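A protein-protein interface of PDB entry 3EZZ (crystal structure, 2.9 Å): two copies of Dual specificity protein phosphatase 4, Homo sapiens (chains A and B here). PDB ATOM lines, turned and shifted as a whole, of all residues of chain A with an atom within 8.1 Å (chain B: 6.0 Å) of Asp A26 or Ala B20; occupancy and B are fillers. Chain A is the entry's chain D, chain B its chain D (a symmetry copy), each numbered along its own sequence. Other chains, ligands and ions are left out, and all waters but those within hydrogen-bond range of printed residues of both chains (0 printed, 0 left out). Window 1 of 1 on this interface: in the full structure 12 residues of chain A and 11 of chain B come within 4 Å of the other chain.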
ATOM      1  N   HIS A  18      -7.197 -12.589   1.079  1.00  0.00           N
ATOM      2  CA  HIS A  18      -6.680 -11.335   0.546  1.00  0.00           C
ATOM      3  C   HIS A  18      -6.875 -10.193   1.529  1.00  0.00           C
ATOM      4  O   HIS A  18      -6.008  -9.336   1.701  1.00  0.00           O
ATOM      5  CB  HIS A  18      -7.401 -11.015  -0.759  1.00  0.00           C
ATOM      6  CG  HIS A  18      -7.288 -12.097  -1.783  1.00  0.00           C
ATOM      7  ND1 HIS A  18      -8.005 -12.087  -2.964  1.00  0.00           N
ATOM      8  CD2 HIS A  18      -6.515 -13.210  -1.822  1.00  0.00           C
ATOM      9  CE1 HIS A  18      -7.675 -13.143  -3.688  1.00  0.00           C
ATOM     10  NE2 HIS A  18      -6.772 -13.841  -3.018  1.00  0.00           N
ATOM     11  N   ARG A  21      -4.177  -9.534   3.834  1.00  0.00           N
ATOM     12  CA  ARG A  21      -2.888  -9.204   3.248  1.00  0.00           C
ATOM     13  C   ARG A  21      -2.709  -7.734   2.918  1.00  0.00           C
ATOM     14  O   ARG A  21      -3.166  -7.257   1.883  1.00  0.00           O
ATOM     15  CB  ARG A  21      -2.688 -10.027   1.983  1.00  0.00           C
ATOM     16  CG  ARG A  21      -2.735 -11.520   2.219  1.00  0.00           C
ATOM     17  CD  ARG A  21      -1.565 -11.961   3.066  1.00  0.00           C
ATOM     18  NE  ARG A  21      -0.289 -11.604   2.447  1.00  0.00           N
ATOM     19  CZ  ARG A  21       0.501 -12.458   1.800  1.00  0.00           C
ATOM     20  NH1 ARG A  21       0.156 -13.737   1.685  1.00  0.00           N
ATOM     21  NH2 ARG A  21       1.637 -12.025   1.260  1.00  0.00           N
ATOM     22  N   ARG A  22      -2.025  -7.017   3.796  1.00  0.00           N
ATOM     23  CA  ARG A  22      -1.776  -5.599   3.574  1.00  0.00           C
ATOM     24  C   ARG A  22      -0.983  -5.389   2.310  1.00  0.00           C
ATOM     25  O   ARG A  22      -1.342  -4.562   1.498  1.00  0.00           O
ATOM     26  CB  ARG A  22      -1.009  -5.004   4.750  1.00  0.00           C
ATOM     27  CG  ARG A  22      -1.913  -4.355   5.771  1.00  0.00           C
ATOM     28  CD  ARG A  22      -1.187  -4.100   7.071  1.00  0.00           C
ATOM     29  NE  ARG A  22      -0.711  -5.347   7.648  1.00  0.00           N
ATOM     30  CZ  ARG A  22      -0.292  -5.467   8.895  1.00  0.00           C
ATOM     31  NH1 ARG A  22      -0.294  -4.408   9.686  1.00  0.00           N
ATOM     32  NH2 ARG A  22       0.120  -6.640   9.347  1.00  0.00           N
ATOM     33  N   ASP A  23       0.108  -6.137   2.159  1.00  0.00           N
ATOM     34  CA  ASP A  23       0.950  -6.030   0.977  1.00  0.00           C
ATOM     35  C   ASP A  23       0.123  -6.111  -0.295  1.00  0.00           C
ATOM     36  O   ASP A  23       0.306  -5.312  -1.218  1.00  0.00           O
ATOM     37  CB  ASP A  23       2.006  -7.136   0.964  1.00  0.00           C
ATOM     38  CG  ASP A  23       1.439  -8.520   1.297  1.00  0.00           C
ATOM     39  OD1 ASP A  23       0.216  -8.714   1.231  1.00  0.00           O
ATOM     40  OD2 ASP A  23       2.229  -9.432   1.619  1.00  0.00           O
ATOM     41  N   MET A  24      -0.785  -7.084  -0.333  1.00  0.00           N
ATOM     42  CA  MET A  24      -1.667  -7.291  -1.482  1.00  0.00           C
ATOM     43  C   MET A  24      -2.624  -6.124  -1.643  1.00  0.00           C
ATOM     44  O   MET A  24      -2.820  -5.631  -2.754  1.00  0.00           O
ATOM     45  CB  MET A  24      -2.470  -8.583  -1.312  1.00  0.00           C
ATOM     46  CG  MET A  24      -1.683  -9.847  -1.616  1.00  0.00           C
ATOM     47  SD  MET A  24      -2.596 -11.344  -1.192  1.00  0.00           S
ATOM     48  CE  MET A  24      -3.893 -11.290  -2.352  1.00  0.00           C
ATOM     49  N   LEU A  25      -3.211  -5.686  -0.530  1.00  0.00           N
ATOM     50  CA  LEU A  25      -4.149  -4.567  -0.530  1.00  0.00           C
ATOM     51  C   LEU A  25      -3.538  -3.252  -1.050  1.00  0.00           C
ATOM     52  O   LEU A  25      -4.121  -2.574  -1.896  1.00  0.00           O
ATOM     53  CB  LEU A  25      -4.675  -4.355   0.884  1.00  0.00           C
ATOM     54  CG  LEU A  25      -5.472  -5.494   1.517  1.00  0.00           C
ATOM     55  CD1 LEU A  25      -5.576  -5.270   3.003  1.00  0.00           C
ATOM     56  CD2 LEU A  25      -6.849  -5.570   0.906  1.00  0.00           C
ATOM     57  N   ASP A  26      -2.361  -2.900  -0.539  1.00  0.00           N
ATOM     58  CA  ASP A  26      -1.683  -1.674  -0.936  1.00  0.00           C
ATOM     59  C   ASP A  26      -1.084  -1.730  -2.325  1.00  0.00           C
ATOM     60  O   ASP A  26      -0.959  -0.700  -2.991  1.00  0.00           O
ATOM     61  CB  ASP A  26      -0.592  -1.345   0.068  1.00  0.00           C
ATOM     62  CG  ASP A  26      -1.134  -1.185   1.457  1.00  0.00           C
ATOM     63  OD1 ASP A  26      -2.274  -0.692   1.581  1.00  0.00           O
ATOM     64  OD2 ASP A  26      -0.423  -1.539   2.414  1.00  0.00           O
ATOM     65  N   ALA A  27      -0.698  -2.929  -2.750  1.00  0.00           N
ATOM     66  CA  ALA A  27      -0.124  -3.129  -4.082  1.00  0.00           C
ATOM     67  C   ALA A  27      -1.195  -2.816  -5.133  1.00  0.00           C
ATOM     68  O   ALA A  27      -0.895  -2.358  -6.234  1.00  0.00           O
ATOM     69  CB  ALA A  27       0.363  -4.564  -4.227  1.00  0.00           C
ATOM     70  N   LEU A  28      -2.448  -3.064  -4.769  1.00  0.00           N
ATOM     71  CA  LEU A  28      -3.576  -2.786  -5.641  1.00  0.00           C
ATOM     72  C   LEU A  28      -4.171  -1.427  -5.312  1.00  0.00           C
ATOM     73  O   LEU A  28      -5.065  -0.943  -6.016  1.00  0.00           O
ATOM     74  CB  LEU A  28      -4.667  -3.836  -5.473  1.00  0.00           C
ATOM     75  CG  LEU A  28      -4.463  -5.098  -6.293  1.00  0.00           C
ATOM     76  CD1 LEU A  28      -5.651  -6.024  -6.098  1.00  0.00           C
ATOM     77  CD2 LEU A  28      -4.312  -4.723  -7.761  1.00  0.00           C
ATOM     78  N   GLY A  29      -3.693  -0.817  -4.235  1.00  0.00           N
ATOM     79  CA  GLY A  29      -4.210   0.479  -3.854  1.00  0.00           C
ATOM     80  C   GLY A  29      -5.646   0.402  -3.376  1.00  0.00           C
ATOM     81  O   GLY A  29      -6.447   1.296  -3.630  1.00  0.00           O
ATOM     82  N   ILE A  30      -5.996  -0.677  -2.700  1.00  0.00           N
ATOM     83  CA  ILE A  30      -7.344  -0.794  -2.178  1.00  0.00           C
ATOM     84  C   ILE A  30      -7.422   0.178  -1.010  1.00  0.00           C
ATOM     85  O   ILE A  30      -6.496   0.253  -0.200  1.00  0.00           O
ATOM     86  CB  ILE A  30      -7.620  -2.211  -1.653  1.00  0.00           C
ATOM     87  CG1 ILE A  30      -7.438  -3.220  -2.783  1.00  0.00           C
ATOM     88  CG2 ILE A  30      -9.021  -2.293  -1.068  1.00  0.00           C
ATOM     89  CD1 ILE A  30      -8.388  -3.029  -3.939  1.00  0.00           C
ATOM     90  N   THR A  31      -8.508   0.935  -0.911  1.00  0.00           N
ATOM     91  CA  THR A  31      -8.652   1.884   0.188  1.00  0.00           C
ATOM     92  C   THR A  31      -9.752   1.435   1.135  1.00  0.00           C
ATOM     93  O   THR A  31      -9.696   1.688   2.328  1.00  0.00           O
ATOM     94  CB  THR A  31      -8.992   3.293  -0.326  1.00  0.00           C
ATOM     95  OG1 THR A  31     -10.362   3.338  -0.736  1.00  0.00           O
ATOM     96  CG2 THR A  31      -8.104   3.651  -1.502  1.00  0.00           C
ATOM     97  N   HIS A  47      -6.269   1.521   9.223  1.00  0.00           N
ATOM     98  CA  HIS A  47      -5.815   1.998   7.919  1.00  0.00           C
ATOM     99  C   HIS A  47      -6.722   1.849   6.716  1.00  0.00           C
ATOM    100  O   HIS A  47      -6.502   2.512   5.706  1.00  0.00           O
ATOM    101  CB  HIS A  47      -4.465   1.377   7.584  1.00  0.00           C
ATOM    102  CG  HIS A  47      -3.470   1.480   8.693  1.00  0.00           C
ATOM    103  ND1 HIS A  47      -3.528   0.685   9.819  1.00  0.00           N
ATOM    104  CD2 HIS A  47      -2.415   2.310   8.873  1.00  0.00           C
ATOM    105  CE1 HIS A  47      -2.554   1.021  10.644  1.00  0.00           C
ATOM    106  NE2 HIS A  47      -1.865   2.004  10.094  1.00  0.00           N
ATOM    107  N   TYR A  48      -7.724   0.986   6.792  1.00  0.00           N
ATOM    108  CA  TYR A  48      -8.608   0.831   5.651  1.00  0.00           C
ATOM    109  C   TYR A  48     -10.045   1.025   6.064  1.00  0.00           C
ATOM    110  O   TYR A  48     -10.400   0.735   7.197  1.00  0.00           O
ATOM    111  CB  TYR A  48      -8.454  -0.553   5.014  1.00  0.00           C
ATOM    112  CG  TYR A  48      -7.033  -0.927   4.652  1.00  0.00           C
ATOM    113  CD1 TYR A  48      -6.180  -1.495   5.601  1.00  0.00           C
ATOM    114  CD2 TYR A  48      -6.531  -0.701   3.364  1.00  0.00           C
ATOM    115  CE1 TYR A  48      -4.856  -1.831   5.276  1.00  0.00           C
ATOM    116  CE2 TYR A  48      -5.202  -1.033   3.031  1.00  0.00           C
ATOM    117  CZ  TYR A  48      -4.377  -1.595   3.992  1.00  0.00           C
ATOM    118  OH  TYR A  48      -3.077  -1.908   3.669  1.00  0.00           O
ATOM    119  N   ARG A  83     -10.822   2.467  -3.948  1.00  0.00           N
ATOM    120  CA  ARG A  83     -10.896   1.121  -4.492  1.00  0.00           C
ATOM    121  C   ARG A  83     -11.403   0.172  -3.422  1.00  0.00           C
ATOM    122  O   ARG A  83     -10.770   0.001  -2.392  1.00  0.00           O
ATOM    123  CB  ARG A  83      -9.527   0.670  -4.989  1.00  0.00           C
ATOM    124  CG  ARG A  83      -8.993   1.459  -6.174  1.00  0.00           C
ATOM    125  CD  ARG A  83      -8.040   0.585  -6.972  1.00  0.00           C
ATOM    126  NE  ARG A  83      -7.485   1.254  -8.144  1.00  0.00           N
ATOM    127  CZ  ARG A  83      -6.520   2.166  -8.098  1.00  0.00           C
ATOM    128  NH1 ARG A  83      -5.997   2.521  -6.931  1.00  0.00           N
ATOM    129  NH2 ARG A  83      -6.077   2.725  -9.221  1.00  0.00           N
ATOM    130  N   SER B  15       7.895  -1.118  -4.329  1.00  0.00           N
ATOM    131  CA  SER B  15       6.434  -1.130  -4.461  1.00  0.00           C
ATOM    132  C   SER B  15       5.767  -0.876  -3.112  1.00  0.00           C
ATOM    133  O   SER B  15       6.417  -0.978  -2.062  1.00  0.00           O
ATOM    134  CB  SER B  15       5.994  -2.502  -4.992  1.00  0.00           C
ATOM    135  OG  SER B  15       4.596  -2.689  -4.902  1.00  0.00           O
ATOM    136  N   ALA B  16       4.477  -0.554  -3.132  1.00  0.00           N
ATOM    137  CA  ALA B  16       3.747  -0.327  -1.888  1.00  0.00           C
ATOM    138  C   ALA B  16       3.580  -1.686  -1.194  1.00  0.00           C
ATOM    139  O   ALA B  16       3.336  -1.780   0.023  1.00  0.00           O
ATOM    140  CB  ALA B  16       2.392   0.281  -2.185  1.00  0.00           C
ATOM    141  N   TYR B  17       3.712  -2.735  -2.003  1.00  0.00           N
ATOM    142  CA  TYR B  17       3.609  -4.108  -1.548  1.00  0.00           C
ATOM    143  C   TYR B  17       4.765  -4.325  -0.582  1.00  0.00           C
ATOM    144  O   TYR B  17       4.608  -4.922   0.486  1.00  0.00           O
ATOM    145  CB  TYR B  17       3.760  -5.049  -2.739  1.00  0.00           C
ATOM    146  CG  TYR B  17       3.715  -6.525  -2.389  1.00  0.00           C
ATOM    147  CD1 TYR B  17       2.542  -7.265  -2.537  1.00  0.00           C
ATOM    148  CD2 TYR B  17       4.843  -7.187  -1.917  1.00  0.00           C
ATOM    149  CE1 TYR B  17       2.496  -8.630  -2.223  1.00  0.00           C
ATOM    150  CE2 TYR B  17       4.802  -8.553  -1.600  1.00  0.00           C
ATOM    151  CZ  TYR B  17       3.629  -9.266  -1.757  1.00  0.00           C
ATOM    152  OH  TYR B  17       3.599 -10.610  -1.456  1.00  0.00           O
ATOM    153  N   HIS B  18       5.930  -3.823  -0.972  1.00  0.00           N
ATOM    154  CA  HIS B  18       7.138  -3.949  -0.168  1.00  0.00           C
ATOM    155  C   HIS B  18       7.009  -3.200   1.147  1.00  0.00           C
ATOM    156  O   HIS B  18       7.445  -3.667   2.201  1.00  0.00           O
ATOM    157  CB  HIS B  18       8.321  -3.394  -0.957  1.00  0.00           C
ATOM    158  CG  HIS B  18       8.512  -4.052  -2.285  1.00  0.00           C
ATOM    159  ND1 HIS B  18       9.411  -3.591  -3.226  1.00  0.00           N
ATOM    160  CD2 HIS B  18       7.945  -5.162  -2.819  1.00  0.00           C
ATOM    161  CE1 HIS B  18       9.393  -4.388  -4.280  1.00  0.00           C
ATOM    162  NE2 HIS B  18       8.513  -5.351  -4.059  1.00  0.00           N
ATOM    163  N   ALA B  19       6.411  -2.022   1.067  1.00  0.00           N
ATOM    164  CA  ALA B  19       6.223  -1.187   2.235  1.00  0.00           C
ATOM    165  C   ALA B  19       5.437  -1.915   3.313  1.00  0.00           C
ATOM    166  O   ALA B  19       5.568  -1.591   4.496  1.00  0.00           O
ATOM    167  CB  ALA B  19       5.502   0.100   1.845  1.00  0.00           C
ATOM    168  N   ALA B  20       4.620  -2.888   2.912  1.00  0.00           N
ATOM    169  CA  ALA B  20       3.809  -3.627   3.870  1.00  0.00           C
ATOM    170  C   ALA B  20       4.512  -4.871   4.392  1.00  0.00           C
ATOM    171  O   ALA B  20       3.940  -5.635   5.171  1.00  0.00           O
ATOM    172  CB  ALA B  20       2.483  -4.006   3.235  1.00  0.00           C
ATOM    173  N   ARG B  21       5.757  -5.060   3.976  1.00  0.00           N
ATOM    174  CA  ARG B  21       6.521  -6.229   4.374  1.00  0.00           C
ATOM    175  C   ARG B  21       7.669  -5.934   5.321  1.00  0.00           C
ATOM    176  O   ARG B  21       8.746  -5.522   4.902  1.00  0.00           O
ATOM    177  CB  ARG B  21       7.067  -6.919   3.131  1.00  0.00           C
ATOM    178  CG  ARG B  21       5.991  -7.360   2.163  1.00  0.00           C
ATOM    179  CD  ARG B  21       5.141  -8.447   2.775  1.00  0.00           C
ATOM    180  NE  ARG B  21       5.947  -9.602   3.169  1.00  0.00           N
ATOM    181  CZ  ARG B  21       6.023 -10.740   2.483  1.00  0.00           C
ATOM    182  NH1 ARG B  21       5.333 -10.891   1.356  1.00  0.00           N
ATOM    183  NH2 ARG B  21       6.800 -11.725   2.924  1.00  0.00           N
ATOM    184  N   ARG B  22       7.440  -6.162   6.606  1.00  0.00           N
ATOM    185  CA  ARG B  22       8.475  -5.930   7.604  1.00  0.00           C
ATOM    186  C   ARG B  22       9.676  -6.801   7.338  1.00  0.00           C
ATOM    187  O   ARG B  22      10.789  -6.318   7.337  1.00  0.00           O
ATOM    188  CB  ARG B  22       7.942  -6.227   9.001  1.00  0.00           C
ATOM    189  CG  ARG B  22       7.435  -4.993   9.710  1.00  0.00           C
ATOM    190  CD  ARG B  22       6.598  -5.350  10.915  1.00  0.00           C
ATOM    191  NE  ARG B  22       5.435  -6.128  10.521  1.00  0.00           N
ATOM    192  CZ  ARG B  22       4.396  -6.344  11.307  1.00  0.00           C
ATOM    193  NH1 ARG B  22       4.386  -5.835  12.526  1.00  0.00           N
ATOM    194  NH2 ARG B  22       3.371  -7.059  10.871  1.00  0.00           N
ATOM    195  N   ASP B  23       9.440  -8.094   7.126  1.00  0.00           N
ATOM    196  CA  ASP B  23      10.517  -9.033   6.852  1.00  0.00           C
ATOM    197  C   ASP B  23      11.426  -8.517   5.750  1.00  0.00           C
ATOM    198  O   ASP B  23      12.654  -8.561   5.873  1.00  0.00           O
ATOM    199  CB  ASP B  23       9.956 -10.396   6.446  1.00  0.00           C
ATOM    200  CG  ASP B  23       8.826 -10.304   5.414  1.00  0.00           C
ATOM    201  OD1 ASP B  23       8.670  -9.258   4.767  1.00  0.00           O
ATOM    202  OD2 ASP B  23       8.090 -11.298   5.238  1.00  0.00           O
ATOM    203  N   LEU B  25      11.609  -5.338   4.648  1.00  0.00           N
ATOM    204  CA  LEU B  25      12.198  -4.081   5.100  1.00  0.00           C
ATOM    205  C   LEU B  25      13.439  -4.270   5.992  1.00  0.00           C
ATOM    206  O   LEU B  25      14.474  -3.639   5.778  1.00  0.00           O
ATOM    207  CB  LEU B  25      11.147  -3.281   5.861  1.00  0.00           C
ATOM    208  CG  LEU B  25       9.904  -2.841   5.090  1.00  0.00           C
ATOM    209  CD1 LEU B  25       8.835  -2.414   6.061  1.00  0.00           C
ATOM    210  CD2 LEU B  25      10.243  -1.704   4.158  1.00  0.00           C
ATOM    211  N   ASP B  39      -2.437   7.582  -0.515  1.00  0.00           N
ATOM    212  CA  ASP B  39      -3.272   6.875   0.459  1.00  0.00           C
ATOM    213  C   ASP B  39      -2.706   5.594   1.030  1.00  0.00           C
ATOM    214  O   ASP B  39      -3.353   4.955   1.860  1.00  0.00           O
ATOM    215  CB  ASP B  39      -4.652   6.575  -0.133  1.00  0.00           C
ATOM    216  CG  ASP B  39      -4.707   6.810  -1.633  1.00  0.00           C
ATOM    217  OD1 ASP B  39      -4.520   7.978  -2.051  1.00  0.00           O
ATOM    218  OD2 ASP B  39      -4.934   5.837  -2.392  1.00  0.00           O
ATOM    219  N   CYS B  40      -1.518   5.198   0.592  1.00  0.00           N
ATOM    220  CA  CYS B  40      -0.929   3.981   1.134  1.00  0.00           C
ATOM    221  C   CYS B  40      -0.675   4.221   2.624  1.00  0.00           C
ATOM    222  O   CYS B  40      -0.016   5.192   3.004  1.00  0.00           O
ATOM    223  CB  CYS B  40       0.384   3.647   0.423  1.00  0.00           C
ATOM    224  SG  CYS B  40       1.150   2.107   0.984  1.00  0.00           S
ATOM    225  N   PRO B  41      -1.213   3.346   3.491  1.00  0.00           N
ATOM    226  CA  PRO B  41      -1.015   3.516   4.934  1.00  0.00           C
ATOM    227  C   PRO B  41       0.435   3.356   5.387  1.00  0.00           C
ATOM    228  O   PRO B  41       1.315   2.934   4.622  1.00  0.00           O
ATOM    229  CB  PRO B  41      -1.916   2.437   5.539  1.00  0.00           C
ATOM    230  CG  PRO B  41      -2.984   2.252   4.500  1.00  0.00           C
ATOM    231  CD  PRO B  41      -2.185   2.272   3.220  1.00  0.00           C
ATOM    232  N   HIS B  43       1.538   1.447   8.161  1.00  0.00           N
ATOM    233  CA  HIS B  43       1.192   0.457   9.155  1.00  0.00           C
ATOM    234  C   HIS B  43       2.084   0.379  10.372  1.00  0.00           C
ATOM    235  O   HIS B  43       1.591   0.265  11.486  1.00  0.00           O
ATOM    236  CB  HIS B  43       1.137  -0.904   8.483  1.00  0.00           C
ATOM    237  CG  HIS B  43       0.295  -0.922   7.245  1.00  0.00           C
ATOM    238  ND1 HIS B  43      -1.084  -0.843   7.282  1.00  0.00           N
ATOM    239  CD2 HIS B  43       0.634  -0.976   5.932  1.00  0.00           C
ATOM    240  CE1 HIS B  43      -1.554  -0.850   6.048  1.00  0.00           C
ATOM    241  NE2 HIS B  43      -0.533  -0.929   5.211  1.00  0.00           N
ATOM    242  N   PHE B  44       3.394   0.452  10.165  1.00  0.00           N
ATOM    243  CA  PHE B  44       4.355   0.334  11.262  1.00  0.00           C
ATOM    244  C   PHE B  44       4.924   1.653  11.732  1.00  0.00           C
ATOM    245  O   PHE B  44       6.131   1.786  11.940  1.00  0.00           O
ATOM    246  CB  PHE B  44       5.465  -0.610  10.828  1.00  0.00           C
ATOM    247  CG  PHE B  44       4.973  -1.685   9.907  1.00  0.00           C
ATOM    248  CD1 PHE B  44       5.198  -1.601   8.536  1.00  0.00           C
ATOM    249  CD2 PHE B  44       4.201  -2.735  10.394  1.00  0.00           C
ATOM    250  CE1 PHE B  44       4.656  -2.538   7.673  1.00  0.00           C
ATOM    251  CE2 PHE B  44       3.656  -3.676   9.532  1.00  0.00           C
ATOM    252  CZ  PHE B  44       3.885  -3.579   8.174  1.00  0.00           C
ATOM    253  N   GLN B  89       2.523   2.964  -5.237  1.00  0.00           N
ATOM    254  CA  GLN B  89       1.726   1.760  -5.527  1.00  0.00           C
ATOM    255  C   GLN B  89       2.431   0.626  -6.270  1.00  0.00           C
ATOM    256  O   GLN B  89       2.620  -0.458  -5.721  1.00  0.00           O
ATOM    257  CB  GLN B  89       0.455   2.107  -6.298  1.00  0.00           C
ATOM    258  CG  GLN B  89      -0.306   0.868  -6.731  1.00  0.00           C
ATOM    259  CD  GLN B  89      -1.789   1.107  -6.884  1.00  0.00           C
ATOM    260  OE1 GLN B  89      -2.533   0.207  -7.242  1.00  0.00           O
ATOM    261  NE2 GLN B  89      -2.230   2.322  -6.605  1.00  0.00           N
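N of Gly A29 lies within hydrogen-bond range of OE1 of Gln B89, at 3.4 Å.
O of Ala A27 sits close to OE1 of Gln B89 (3.2 Å).
The side-chain carboxylate of Asp A23 is in salt-bridge range of the guanidinium group of Arg B21 (3.4 Å).
The side-chain carboxylate (OD2) of Asp A26 is in hydrogen-bond range of a ring nitrogen (NE2) of His B43 (2.9 Å).
The backbone carbonyl oxygen of Leu A28 sits close to the side-chain amide oxygen of Gln B89, at 3.0 Å.
OH of Tyr A48 lies close to NE2 of His B43, 3.1 Å away.
OG of Ser B15 lies within hydrogen-bond range of O of Gln B89, 3.1 Å away.
The side-chain carboxylate (OD1) of Asp A26 lies within hydrogen-bond range of the side-chain hydroxyl (OH) of Tyr A48, at 2.5 Å.
The side-chain hydroxyl (OH) of Tyr B17 sits at hydrogen-bond distance from the guanidinium group (NH1) of Arg B21 (3.3 Å).
The backbone NH (N) of Ala B16 lies within hydrogen-bond range of the backbone carbonyl oxygen (O) of Gln B89, 3.2 Å away.
The guanidinium group (NH2) of Arg B21 is in salt-bridge range of the side-chain carboxylate (OD2) of Asp B23, 2.7 Å away.
The backbone NH (N) of Thr A31 is in hydrogen-bond range of the backbone carbonyl oxygen (O) of Arg A83 (2.9 Å).
NH2 of Arg A21 touches OH of Tyr B17, at 3.6 Å.
Ala B20 touches Arg A22 (CB to C, 3.8 Å).
Met A24 touches Tyr B17 (N to CD1, 3.99 Å).
OD2 of Asp A26 touches CB of Ala B20, 3.9 Å away.
Asp A26 touches Cys B40.
Tyr B17 touches Ala A27 (CB to CB, 3.7 Å).
CG2 of Thr A31 touches OD2 of Asp B39 (3.95 Å).
His A47 touches Pro B41 (CD2 to CB, 3.4 Å).
His A47 touches His B43.
NH1 of Arg A83 touches NE2 of Gln B89 (3.8 Å).
His A18 touches none of the printed residues of chain B.
Of chain B, only Ala B16 (3.6 Å), Ala B20 (3.9 Å), Cys B40 (3.97 Å), Pro B41 (3.4 Å) and His B43 (2.9 Å) come within 4 Å of Asp A26.
Of the printed residues of chain A, Ala B16 touches Asp A26.
No residue of chain A comes within 4 Å of Ala B19.
Ala B20 touches just these residues of chain A: Arg A22, Asp A23 and Asp A26.
Of the printed residues of chain A, Arg B21 touches Arg A21 and Asp A23.
Printed residues of chain A within 4 Å of Asp B39: Thr A31.
Printed residues of chain A that touch a printed residue of chain B: Arg A21, Arg A22, Asp A23, Met A24, Asp A26, Ala A27, Leu A28, Gly A29, Thr A31, His A47, Tyr A48 and Arg A83.
Of the 16 printed residues of chain B, 10 touch a printed residue of chain A.
Among the printed residues, 23 pairs touch across the chains.
Arg B21 touches its own counterpart, Arg A21.
Arg B22 touches its own counterpart, Arg A22.
Asp A23 touches Arg B21, but with the chains exchanged Arg A21 does not touch Asp B23 (7.6 Å).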
